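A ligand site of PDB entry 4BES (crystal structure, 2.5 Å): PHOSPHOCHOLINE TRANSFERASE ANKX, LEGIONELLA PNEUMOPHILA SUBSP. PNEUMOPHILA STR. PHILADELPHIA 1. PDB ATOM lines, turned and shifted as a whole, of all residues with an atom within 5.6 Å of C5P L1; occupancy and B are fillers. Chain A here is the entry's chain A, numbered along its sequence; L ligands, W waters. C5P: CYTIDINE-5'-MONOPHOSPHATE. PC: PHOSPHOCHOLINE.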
ATOM      1  N   PHE A  26      33.224 -16.081 -16.198  1.00  0.00           N
ATOM      2  CA  PHE A  26      32.795 -17.179 -15.327  1.00  0.00           C
ATOM      3  C   PHE A  26      31.270 -17.318 -15.315  1.00  0.00           C
ATOM      4  O   PHE A  26      30.781 -18.439 -15.379  1.00  0.00           O
ATOM      5  CB  PHE A  26      33.377 -17.023 -13.906  1.00  0.00           C
ATOM      6  CG  PHE A  26      34.881 -16.872 -13.932  1.00  0.00           C
ATOM      7  CD1 PHE A  26      35.708 -17.959 -14.228  1.00  0.00           C
ATOM      8  CD2 PHE A  26      35.476 -15.623 -13.758  1.00  0.00           C
ATOM      9  CE1 PHE A  26      37.093 -17.802 -14.326  1.00  0.00           C
ATOM     10  CE2 PHE A  26      36.862 -15.465 -13.856  1.00  0.00           C
ATOM     11  CZ  PHE A  26      37.657 -16.557 -14.136  1.00  0.00           C
ATOM     12  N   ASP A  28      27.685 -17.434 -16.844  1.00  0.00           N
ATOM     13  CA  ASP A  28      27.042 -17.693 -18.152  1.00  0.00           C
ATOM     14  C   ASP A  28      26.125 -16.555 -18.546  1.00  0.00           C
ATOM     15  O   ASP A  28      25.249 -16.174 -17.764  1.00  0.00           O
ATOM     16  CB  ASP A  28      26.203 -18.987 -18.140  1.00  0.00           C
ATOM     17  CG  ASP A  28      26.819 -20.189 -17.487  1.00  0.00           C
ATOM     18  OD1 ASP A  28      28.009 -20.112 -17.074  1.00  0.00           O
ATOM     19  OD2 ASP A  28      26.125 -21.212 -17.380  1.00  0.00           O
ATOM     20  N   ARG A  30      23.584 -16.420 -20.188  1.00  0.00           N
ATOM     21  CA  ARG A  30      22.163 -16.785 -20.079  1.00  0.00           C
ATOM     22  C   ARG A  30      21.515 -16.283 -18.774  1.00  0.00           C
ATOM     23  O   ARG A  30      20.312 -16.113 -18.729  1.00  0.00           O
ATOM     24  CB  ARG A  30      21.979 -18.310 -20.237  1.00  0.00           C
ATOM     25  CG  ARG A  30      22.599 -19.153 -19.125  1.00  0.00           C
ATOM     26  CD  ARG A  30      22.962 -20.533 -19.625  1.00  0.00           C
ATOM     27  NE  ARG A  30      23.587 -21.350 -18.583  1.00  0.00           N
ATOM     28  CZ  ARG A  30      22.925 -22.142 -17.743  1.00  0.00           C
ATOM     29  NH1 ARG A  30      21.604 -22.206 -17.803  1.00  0.00           N
ATOM     30  NH2 ARG A  30      23.572 -22.863 -16.850  1.00  0.00           N
ATOM     31  N   PHE A  31      22.337 -16.077 -17.729  1.00  0.00           N
ATOM     32  CA  PHE A  31      21.919 -15.667 -16.382  1.00  0.00           C
ATOM     33  C   PHE A  31      21.809 -14.166 -16.200  1.00  0.00           C
ATOM     34  O   PHE A  31      21.028 -13.715 -15.355  1.00  0.00           O
ATOM     35  CB  PHE A  31      22.949 -16.147 -15.365  1.00  0.00           C
ATOM     36  CG  PHE A  31      23.197 -17.633 -15.197  1.00  0.00           C
ATOM     37  CD1 PHE A  31      22.133 -18.528 -15.102  1.00  0.00           C
ATOM     38  CD2 PHE A  31      24.489 -18.117 -14.971  1.00  0.00           C
ATOM     39  CE1 PHE A  31      22.353 -19.878 -14.871  1.00  0.00           C
ATOM     40  CE2 PHE A  31      24.699 -19.466 -14.722  1.00  0.00           C
ATOM     41  CZ  PHE A  31      23.641 -20.339 -14.673  1.00  0.00           C
ATOM     42  N   TYR A  41      24.865 -16.015  -9.409  1.00  0.00           N
ATOM     43  CA  TYR A  41      25.949 -16.995  -9.527  1.00  0.00           C
ATOM     44  C   TYR A  41      26.750 -17.034  -8.212  1.00  0.00           C
ATOM     45  O   TYR A  41      27.028 -18.122  -7.703  1.00  0.00           O
ATOM     46  CB  TYR A  41      26.874 -16.645 -10.704  1.00  0.00           C
ATOM     47  CG  TYR A  41      27.910 -17.690 -11.078  1.00  0.00           C
ATOM     48  CD1 TYR A  41      29.176 -17.680 -10.496  1.00  0.00           C
ATOM     49  CD2 TYR A  41      27.677 -18.596 -12.111  1.00  0.00           C
ATOM     50  CE1 TYR A  41      30.153 -18.602 -10.872  1.00  0.00           C
ATOM     51  CE2 TYR A  41      28.653 -19.514 -12.511  1.00  0.00           C
ATOM     52  CZ  TYR A  41      29.890 -19.521 -11.886  1.00  0.00           C
ATOM     53  OH  TYR A  41      30.870 -20.439 -12.248  1.00  0.00           O
ATOM     54  N   GLU A  42      27.056 -15.824  -7.646  1.00  0.00           N
ATOM     55  CA  GLU A  42      27.786 -15.684  -6.391  1.00  0.00           C
ATOM     56  C   GLU A  42      27.008 -16.212  -5.225  1.00  0.00           C
ATOM     57  O   GLU A  42      27.613 -16.886  -4.398  1.00  0.00           O
ATOM     58  CB  GLU A  42      28.264 -14.257  -6.153  1.00  0.00           C
ATOM     59  CG  GLU A  42      29.779 -14.117  -6.277  1.00  0.00           C
ATOM     60  CD  GLU A  42      30.668 -14.637  -5.154  1.00  0.00           C
ATOM     61  OE1 GLU A  42      30.145 -14.872  -4.040  1.00  0.00           O
ATOM     62  OE2 GLU A  42      31.888 -14.761  -5.369  1.00  0.00           O
ATOM     63  N   ARG A  44      24.763 -18.694  -5.107  1.00  0.00           N
ATOM     64  CA  ARG A  44      24.698 -20.170  -5.186  1.00  0.00           C
ATOM     65  C   ARG A  44      25.901 -20.851  -4.514  1.00  0.00           C
ATOM     66  O   ARG A  44      25.756 -21.951  -3.976  1.00  0.00           O
ATOM     67  CB  ARG A  44      24.581 -20.660  -6.623  1.00  0.00           C
ATOM     68  CG  ARG A  44      23.207 -20.498  -7.217  1.00  0.00           C
ATOM     69  CD  ARG A  44      23.228 -21.011  -8.628  1.00  0.00           C
ATOM     70  NE  ARG A  44      22.504 -20.146  -9.547  1.00  0.00           N
ATOM     71  CZ  ARG A  44      23.070 -19.415 -10.497  1.00  0.00           C
ATOM     72  NH1 ARG A  44      24.381 -19.445 -10.679  1.00  0.00           N
ATOM     73  NH2 ARG A  44      22.335 -18.670 -11.292  1.00  0.00           N
ATOM     74  N   GLU A  45      27.072 -20.219  -4.577  1.00  0.00           N
ATOM     75  CA  GLU A  45      28.314 -20.712  -3.994  1.00  0.00           C
ATOM     76  C   GLU A  45      29.144 -19.470  -3.608  1.00  0.00           C
ATOM     77  O   GLU A  45      29.960 -19.034  -4.414  1.00  0.00           O
ATOM     78  CB  GLU A  45      29.102 -21.590  -4.990  1.00  0.00           C
ATOM     79  CG  GLU A  45      28.498 -22.951  -5.310  1.00  0.00           C
ATOM     80  CD  GLU A  45      29.169 -23.774  -6.394  1.00  0.00           C
ATOM     81  OE1 GLU A  45      30.421 -23.744  -6.489  1.00  0.00           O
ATOM     82  OE2 GLU A  45      28.448 -24.508  -7.104  1.00  0.00           O
ATOM     83  N   CYS A  48      32.875 -18.367  -4.957  1.00  0.00           N
ATOM     84  CA  CYS A  48      33.157 -19.035  -6.230  1.00  0.00           C
ATOM     85  C   CYS A  48      33.670 -18.210  -7.386  1.00  0.00           C
ATOM     86  O   CYS A  48      34.352 -18.763  -8.244  1.00  0.00           O
ATOM     87  CB  CYS A  48      32.037 -19.985  -6.644  1.00  0.00           C
ATOM     88  SG  CYS A  48      30.584 -19.172  -7.350  1.00  0.00           S
ATOM     89  N   ARG A 113      21.152 -28.522 -25.297  1.00  0.00           N
ATOM     90  CA  ARG A 113      22.598 -28.664 -25.082  1.00  0.00           C
ATOM     91  C   ARG A 113      23.158 -29.836 -25.882  1.00  0.00           C
ATOM     92  O   ARG A 113      24.256 -30.338 -25.618  1.00  0.00           O
ATOM     93  CB  ARG A 113      22.877 -28.803 -23.567  1.00  0.00           C
ATOM     94  CG  ARG A 113      22.799 -27.471 -22.811  1.00  0.00           C
ATOM     95  CD  ARG A 113      22.786 -27.743 -21.329  1.00  0.00           C
ATOM     96  NE  ARG A 113      22.771 -26.521 -20.523  1.00  0.00           N
ATOM     97  CZ  ARG A 113      22.859 -26.520 -19.195  1.00  0.00           C
ATOM     98  NH1 ARG A 113      22.962 -27.664 -18.528  1.00  0.00           N
ATOM     99  NH2 ARG A 113      22.867 -25.369 -18.532  1.00  0.00           N
ATOM    100  N   ASP A 233      32.877 -32.674  -8.386  1.00  0.00           N
ATOM    101  CA  ASP A 233      32.280 -31.344  -8.537  1.00  0.00           C
ATOM    102  C   ASP A 233      33.169 -30.489  -9.435  1.00  0.00           C
ATOM    103  O   ASP A 233      34.305 -30.871  -9.710  1.00  0.00           O
ATOM    104  CB  ASP A 233      32.206 -30.677  -7.138  1.00  0.00           C
ATOM    105  CG  ASP A 233      33.563 -30.473  -6.462  1.00  0.00           C
ATOM    106  OD1 ASP A 233      34.381 -31.441  -6.437  1.00  0.00           O
ATOM    107  OD2 ASP A 233      33.818 -29.345  -5.965  1.00  0.00           O
ATOM    108  N   ALA A 234      32.663 -29.333  -9.865  1.00  0.00           N
ATOM    109  CA  ALA A 234      33.364 -28.302 -10.636  1.00  0.00           C
ATOM    110  C   ALA A 234      34.112 -28.730 -11.912  1.00  0.00           C
ATOM    111  O   ALA A 234      35.185 -28.209 -12.198  1.00  0.00           O
ATOM    112  CB  ALA A 234      34.281 -27.491  -9.722  1.00  0.00           C
ATOM    113  N   ASN A 235      33.523 -29.649 -12.688  1.00  0.00           N
ATOM    114  CA  ASN A 235      34.150 -30.098 -13.929  1.00  0.00           C
ATOM    115  C   ASN A 235      34.095 -29.012 -15.007  1.00  0.00           C
ATOM    116  O   ASN A 235      35.083 -28.808 -15.722  1.00  0.00           O
ATOM    117  CB  ASN A 235      33.569 -31.436 -14.390  1.00  0.00           C
ATOM    118  CG  ASN A 235      34.092 -32.617 -13.608  1.00  0.00           C
ATOM    119  OD1 ASN A 235      35.282 -32.935 -13.635  1.00  0.00           O
ATOM    120  ND2 ASN A 235      33.223 -33.294 -12.868  1.00  0.00           N
ATOM    121  N   GLY A 236      32.971 -28.288 -15.074  1.00  0.00           N
ATOM    122  CA  GLY A 236      32.762 -27.195 -16.011  1.00  0.00           C
ATOM    123  C   GLY A 236      33.779 -26.079 -15.851  1.00  0.00           C
ATOM    124  O   GLY A 236      34.504 -25.773 -16.793  1.00  0.00           O
ATOM    125  N   ARG A 237      33.868 -25.516 -14.649  1.00  0.00           N
ATOM    126  CA  ARG A 237      34.805 -24.432 -14.324  1.00  0.00           C
ATOM    127  C   ARG A 237      36.260 -24.808 -14.549  1.00  0.00           C
ATOM    128  O   ARG A 237      37.060 -23.974 -14.972  1.00  0.00           O
ATOM    129  CB  ARG A 237      34.632 -23.967 -12.870  1.00  0.00           C
ATOM    130  CG  ARG A 237      33.477 -22.984 -12.713  1.00  0.00           C
ATOM    131  CD  ARG A 237      33.083 -22.827 -11.257  1.00  0.00           C
ATOM    132  NE  ARG A 237      32.183 -23.889 -10.801  1.00  0.00           N
ATOM    133  CZ  ARG A 237      31.795 -24.055  -9.543  1.00  0.00           C
ATOM    134  NH1 ARG A 237      32.182 -23.197  -8.601  1.00  0.00           N
ATOM    135  NH2 ARG A 237      30.970 -25.047  -9.225  1.00  0.00           N
ATOM    136  N   THR A 238      36.600 -26.059 -14.209  1.00  0.00           N
ATOM    137  CA  THR A 238      37.955 -26.604 -14.290  1.00  0.00           C
ATOM    138  C   THR A 238      38.448 -26.646 -15.722  1.00  0.00           C
ATOM    139  O   THR A 238      39.542 -26.137 -15.994  1.00  0.00           O
ATOM    140  CB  THR A 238      38.028 -27.997 -13.616  1.00  0.00           C
ATOM    141  OG1 THR A 238      37.691 -27.836 -12.242  1.00  0.00           O
ATOM    142  CG2 THR A 238      39.401 -28.676 -13.743  1.00  0.00           C
ATOM    143  N   ASN A 241      36.084 -22.984 -18.136  1.00  0.00           N
ATOM    144  CA  ASN A 241      36.330 -21.610 -17.705  1.00  0.00           C
ATOM    145  C   ASN A 241      37.787 -21.346 -17.314  1.00  0.00           C
ATOM    146  O   ASN A 241      38.200 -20.190 -17.205  1.00  0.00           O
ATOM    147  CB  ASN A 241      35.326 -21.185 -16.617  1.00  0.00           C
ATOM    148  CG  ASN A 241      33.894 -21.259 -17.117  1.00  0.00           C
ATOM    149  OD1 ASN A 241      33.460 -20.459 -17.949  1.00  0.00           O
ATOM    150  ND2 ASN A 241      33.170 -22.295 -16.734  1.00  0.00           N
ATOM    151  N   GLU A 260      26.266 -19.887 -22.915  1.00  0.00           N
ATOM    152  CA  GLU A 260      25.965 -21.237 -22.423  1.00  0.00           C
ATOM    153  C   GLU A 260      27.199 -22.129 -22.589  1.00  0.00           C
ATOM    154  O   GLU A 260      27.457 -22.594 -23.699  1.00  0.00           O
ATOM    155  CB  GLU A 260      24.717 -21.804 -23.173  1.00  0.00           C
ATOM    156  CG  GLU A 260      24.337 -23.250 -22.906  1.00  0.00           C
ATOM    157  CD  GLU A 260      24.044 -23.545 -21.449  1.00  0.00           C
ATOM    158  OE1 GLU A 260      24.988 -23.481 -20.632  1.00  0.00           O
ATOM    159  OE2 GLU A 260      22.849 -23.756 -21.115  1.00  0.00           O
ATOM    160  N   PRO A 261      28.037 -22.297 -21.531  1.00  0.00           N
ATOM    161  CA  PRO A 261      29.264 -23.124 -21.685  1.00  0.00           C
ATOM    162  C   PRO A 261      29.004 -24.622 -21.574  1.00  0.00           C
ATOM    163  O   PRO A 261      29.853 -25.424 -21.933  1.00  0.00           O
ATOM    164  CB  PRO A 261      30.137 -22.663 -20.517  1.00  0.00           C
ATOM    165  CG  PRO A 261      29.158 -22.275 -19.469  1.00  0.00           C
ATOM    166  CD  PRO A 261      27.929 -21.743 -20.166  1.00  0.00           C
ATOM    167  N   ASN A 262      27.830 -24.959 -21.039  1.00  0.00           N
ATOM    168  CA  ASN A 262      27.447 -26.342 -20.768  1.00  0.00           C
ATOM    169  C   ASN A 262      26.994 -27.098 -22.006  1.00  0.00           C
ATOM    170  O   ASN A 262      25.916 -27.687 -22.032  1.00  0.00           O
ATOM    171  CB  ASN A 262      26.359 -26.397 -19.695  1.00  0.00           C
ATOM    172  CG  ASN A 262      26.751 -25.658 -18.422  1.00  0.00           C
ATOM    173  OD1 ASN A 262      27.609 -26.120 -17.674  1.00  0.00           O
ATOM    174  ND2 ASN A 262      26.128 -24.513 -18.184  1.00  0.00           N
HETATM  175  O3P C5P L   1      31.080 -28.075 -13.058  1.00  0.00           O
HETATM  176  P   C5P L   1      30.573 -26.713 -12.655  1.00  0.00           P
HETATM  177  O1P C5P L   1      29.822 -26.697 -11.328  1.00  0.00           O
HETATM  178  O2P C5P L   1      31.788 -25.825 -12.671  1.00  0.00           O
HETATM  179  O5' C5P L   1      29.641 -26.267 -13.866  1.00  0.00           O
HETATM  180  C5' C5P L   1      29.656 -25.042 -14.624  1.00  0.00           C
HETATM  181  C4' C5P L   1      28.269 -24.448 -14.695  1.00  0.00           C
HETATM  182  O4' C5P L   1      27.574 -24.604 -13.435  1.00  0.00           O
HETATM  183  C3' C5P L   1      28.240 -22.952 -14.955  1.00  0.00           C
HETATM  184  O3' C5P L   1      28.410 -22.692 -16.342  1.00  0.00           O
HETATM  185  C2' C5P L   1      26.843 -22.577 -14.449  1.00  0.00           C
HETATM  186  O2' C5P L   1      25.826 -22.919 -15.376  1.00  0.00           O
HETATM  187  C1' C5P L   1      26.725 -23.490 -13.224  1.00  0.00           C
HETATM  188  N1  C5P L   1      27.098 -22.820 -11.955  1.00  0.00           N
HETATM  189  C2  C5P L   1      26.195 -21.882 -11.420  1.00  0.00           C
HETATM  190  N3  C5P L   1      26.521 -21.250 -10.258  1.00  0.00           N
HETATM  191  C4  C5P L   1      27.685 -21.499  -9.640  1.00  0.00           C
HETATM  192  C5  C5P L   1      28.620 -22.438 -10.168  1.00  0.00           C
HETATM  193  C6  C5P L   1      28.297 -23.066 -11.317  1.00  0.00           C
HETATM  194  O2  C5P L   1      25.139 -21.664 -12.016  1.00  0.00           O
HETATM  195  N4  C5P L   1      27.952 -20.849  -8.515  1.00  0.00           N
HETATM  196  P1   PC L   2      29.830 -31.299 -12.047  1.00  0.00           P
HETATM  197  O1   PC L   2      29.449 -30.130 -11.221  1.00  0.00           O
HETATM  198  O3   PC L   2      28.814 -32.451 -11.968  1.00  0.00           O
HETATM  199  O4   PC L   2      31.211 -31.834 -11.727  1.00  0.00           O
HETATM  200  O2   PC L   2      29.874 -30.828 -13.612  1.00  0.00           O
HETATM  201  C1   PC L   2      28.663 -30.440 -14.306  1.00  0.00           C
HETATM  202  C2   PC L   2      29.077 -29.875 -15.647  1.00  0.00           C
HETATM  203  N1   PC L   2      27.987 -29.734 -16.689  1.00  0.00           N
HETATM  204  C3   PC L   2      26.861 -28.877 -16.175  1.00  0.00           C
HETATM  205  C4   PC L   2      27.448 -31.064 -17.079  1.00  0.00           C
HETATM  206  C5   PC L   2      28.584 -29.090 -17.893  1.00  0.00           C
HETATM  207  O   HOH W   1      29.742 -28.607  -9.208  1.00  0.00           O
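Water W1 lies within hydrogen-bond range of an oxygen (O1) of PC L2 (2.5 Å), an oxygen (O1P) of C5P L1 (2.9 Å) and the backbone NH (N) of Ala 234 (3.1 Å).
O4 of PC L2 is in hydrogen-bond range of ND2 of Asn 235, 2.7 Å away.
SG of Cys 48 lies within hydrogen-bond range of N4 of C5P L1 (3.3 Å).
The backbone carbonyl oxygen of Tyr 41 lies within hydrogen-bond range of a nitrogen (N4) of C5P L1.
The backbone NH of Asn 235 sits at hydrogen-bond distance from an oxygen (O3P) of C5P L1, at 2.9 Å.
The guanidinium group (NE) of Arg 237 is in salt-bridge range of an oxygen (O2P) of C5P L1, 2.7 Å away.
O4 of PC L2 is in hydrogen-bond range of N of Ala 234 (3.4 Å).
The side-chain amide nitrogen (ND2) of Asn 262 sits at hydrogen-bond distance from an oxygen (O2') of C5P L1 (3.2 Å).
The guanidinium group of Arg 44 is in hydrogen-bond range of an oxygen (O2) of C5P L1, 2.7 Å away.
An oxygen (O2') of C5P L1 lies within hydrogen-bond range of the side-chain carboxylate (OD2) of Asp 28, at 2.6 Å.
NH2 of Arg 30 lies within hydrogen-bond range of O2' of C5P L1, at 2.7 Å.
An oxygen (O3P) of C5P L1 lies within hydrogen-bond range of the backbone NH of Gly 236, at 2.8 Å.
N of Asn 235 is in hydrogen-bond range of O4 of PC L2, 3.3 Å away.
The backbone NH (N) of Arg 237 lies within hydrogen-bond range of an oxygen (O2P) of C5P L1.
Merely in contact with C5P L1: Pro 261, Ala 234, Phe 31 and Glu 45.
Hydrophobic or aromatic side chains that line C5P L1: Phe 31, Tyr 41 and Pro 261.
The nearest printed residue that does not touch C5P L1 is Asn 241 (4.8 Å).
The guanidinium group (NH2) of Arg 113 sits close to the side-chain amide nitrogen (ND2) of Asn 262.
The side-chain amide nitrogen of Asn 262 sits close to the guanidinium group of Arg 30.
N of Asn 241 sits at hydrogen-bond distance from O of Gly 236 (3.5 Å).
The side-chain hydroxyl of Thr 238 lies within hydrogen-bond range of the backbone carbonyl oxygen of Ala 234 (2.5 Å).
The side-chain carboxylate of Glu 260 lies within hydrogen-bond range of the side-chain amide nitrogen of Asn 262 (2.9 Å).
SG of Cys 48 is in hydrogen-bond range of O of Glu 45 (3.0 Å).
NH1 of Arg 237 lies within salt-bridge range of OE1 of Glu 45 (2.8 Å).
The side-chain amide nitrogen of Asn 262 sits at hydrogen-bond distance from the side-chain carboxylate of Asp 28, at 3.4 Å.
An oxygen (O3P) of C5P L1 lies close to an oxygen (O2) of PC L2.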
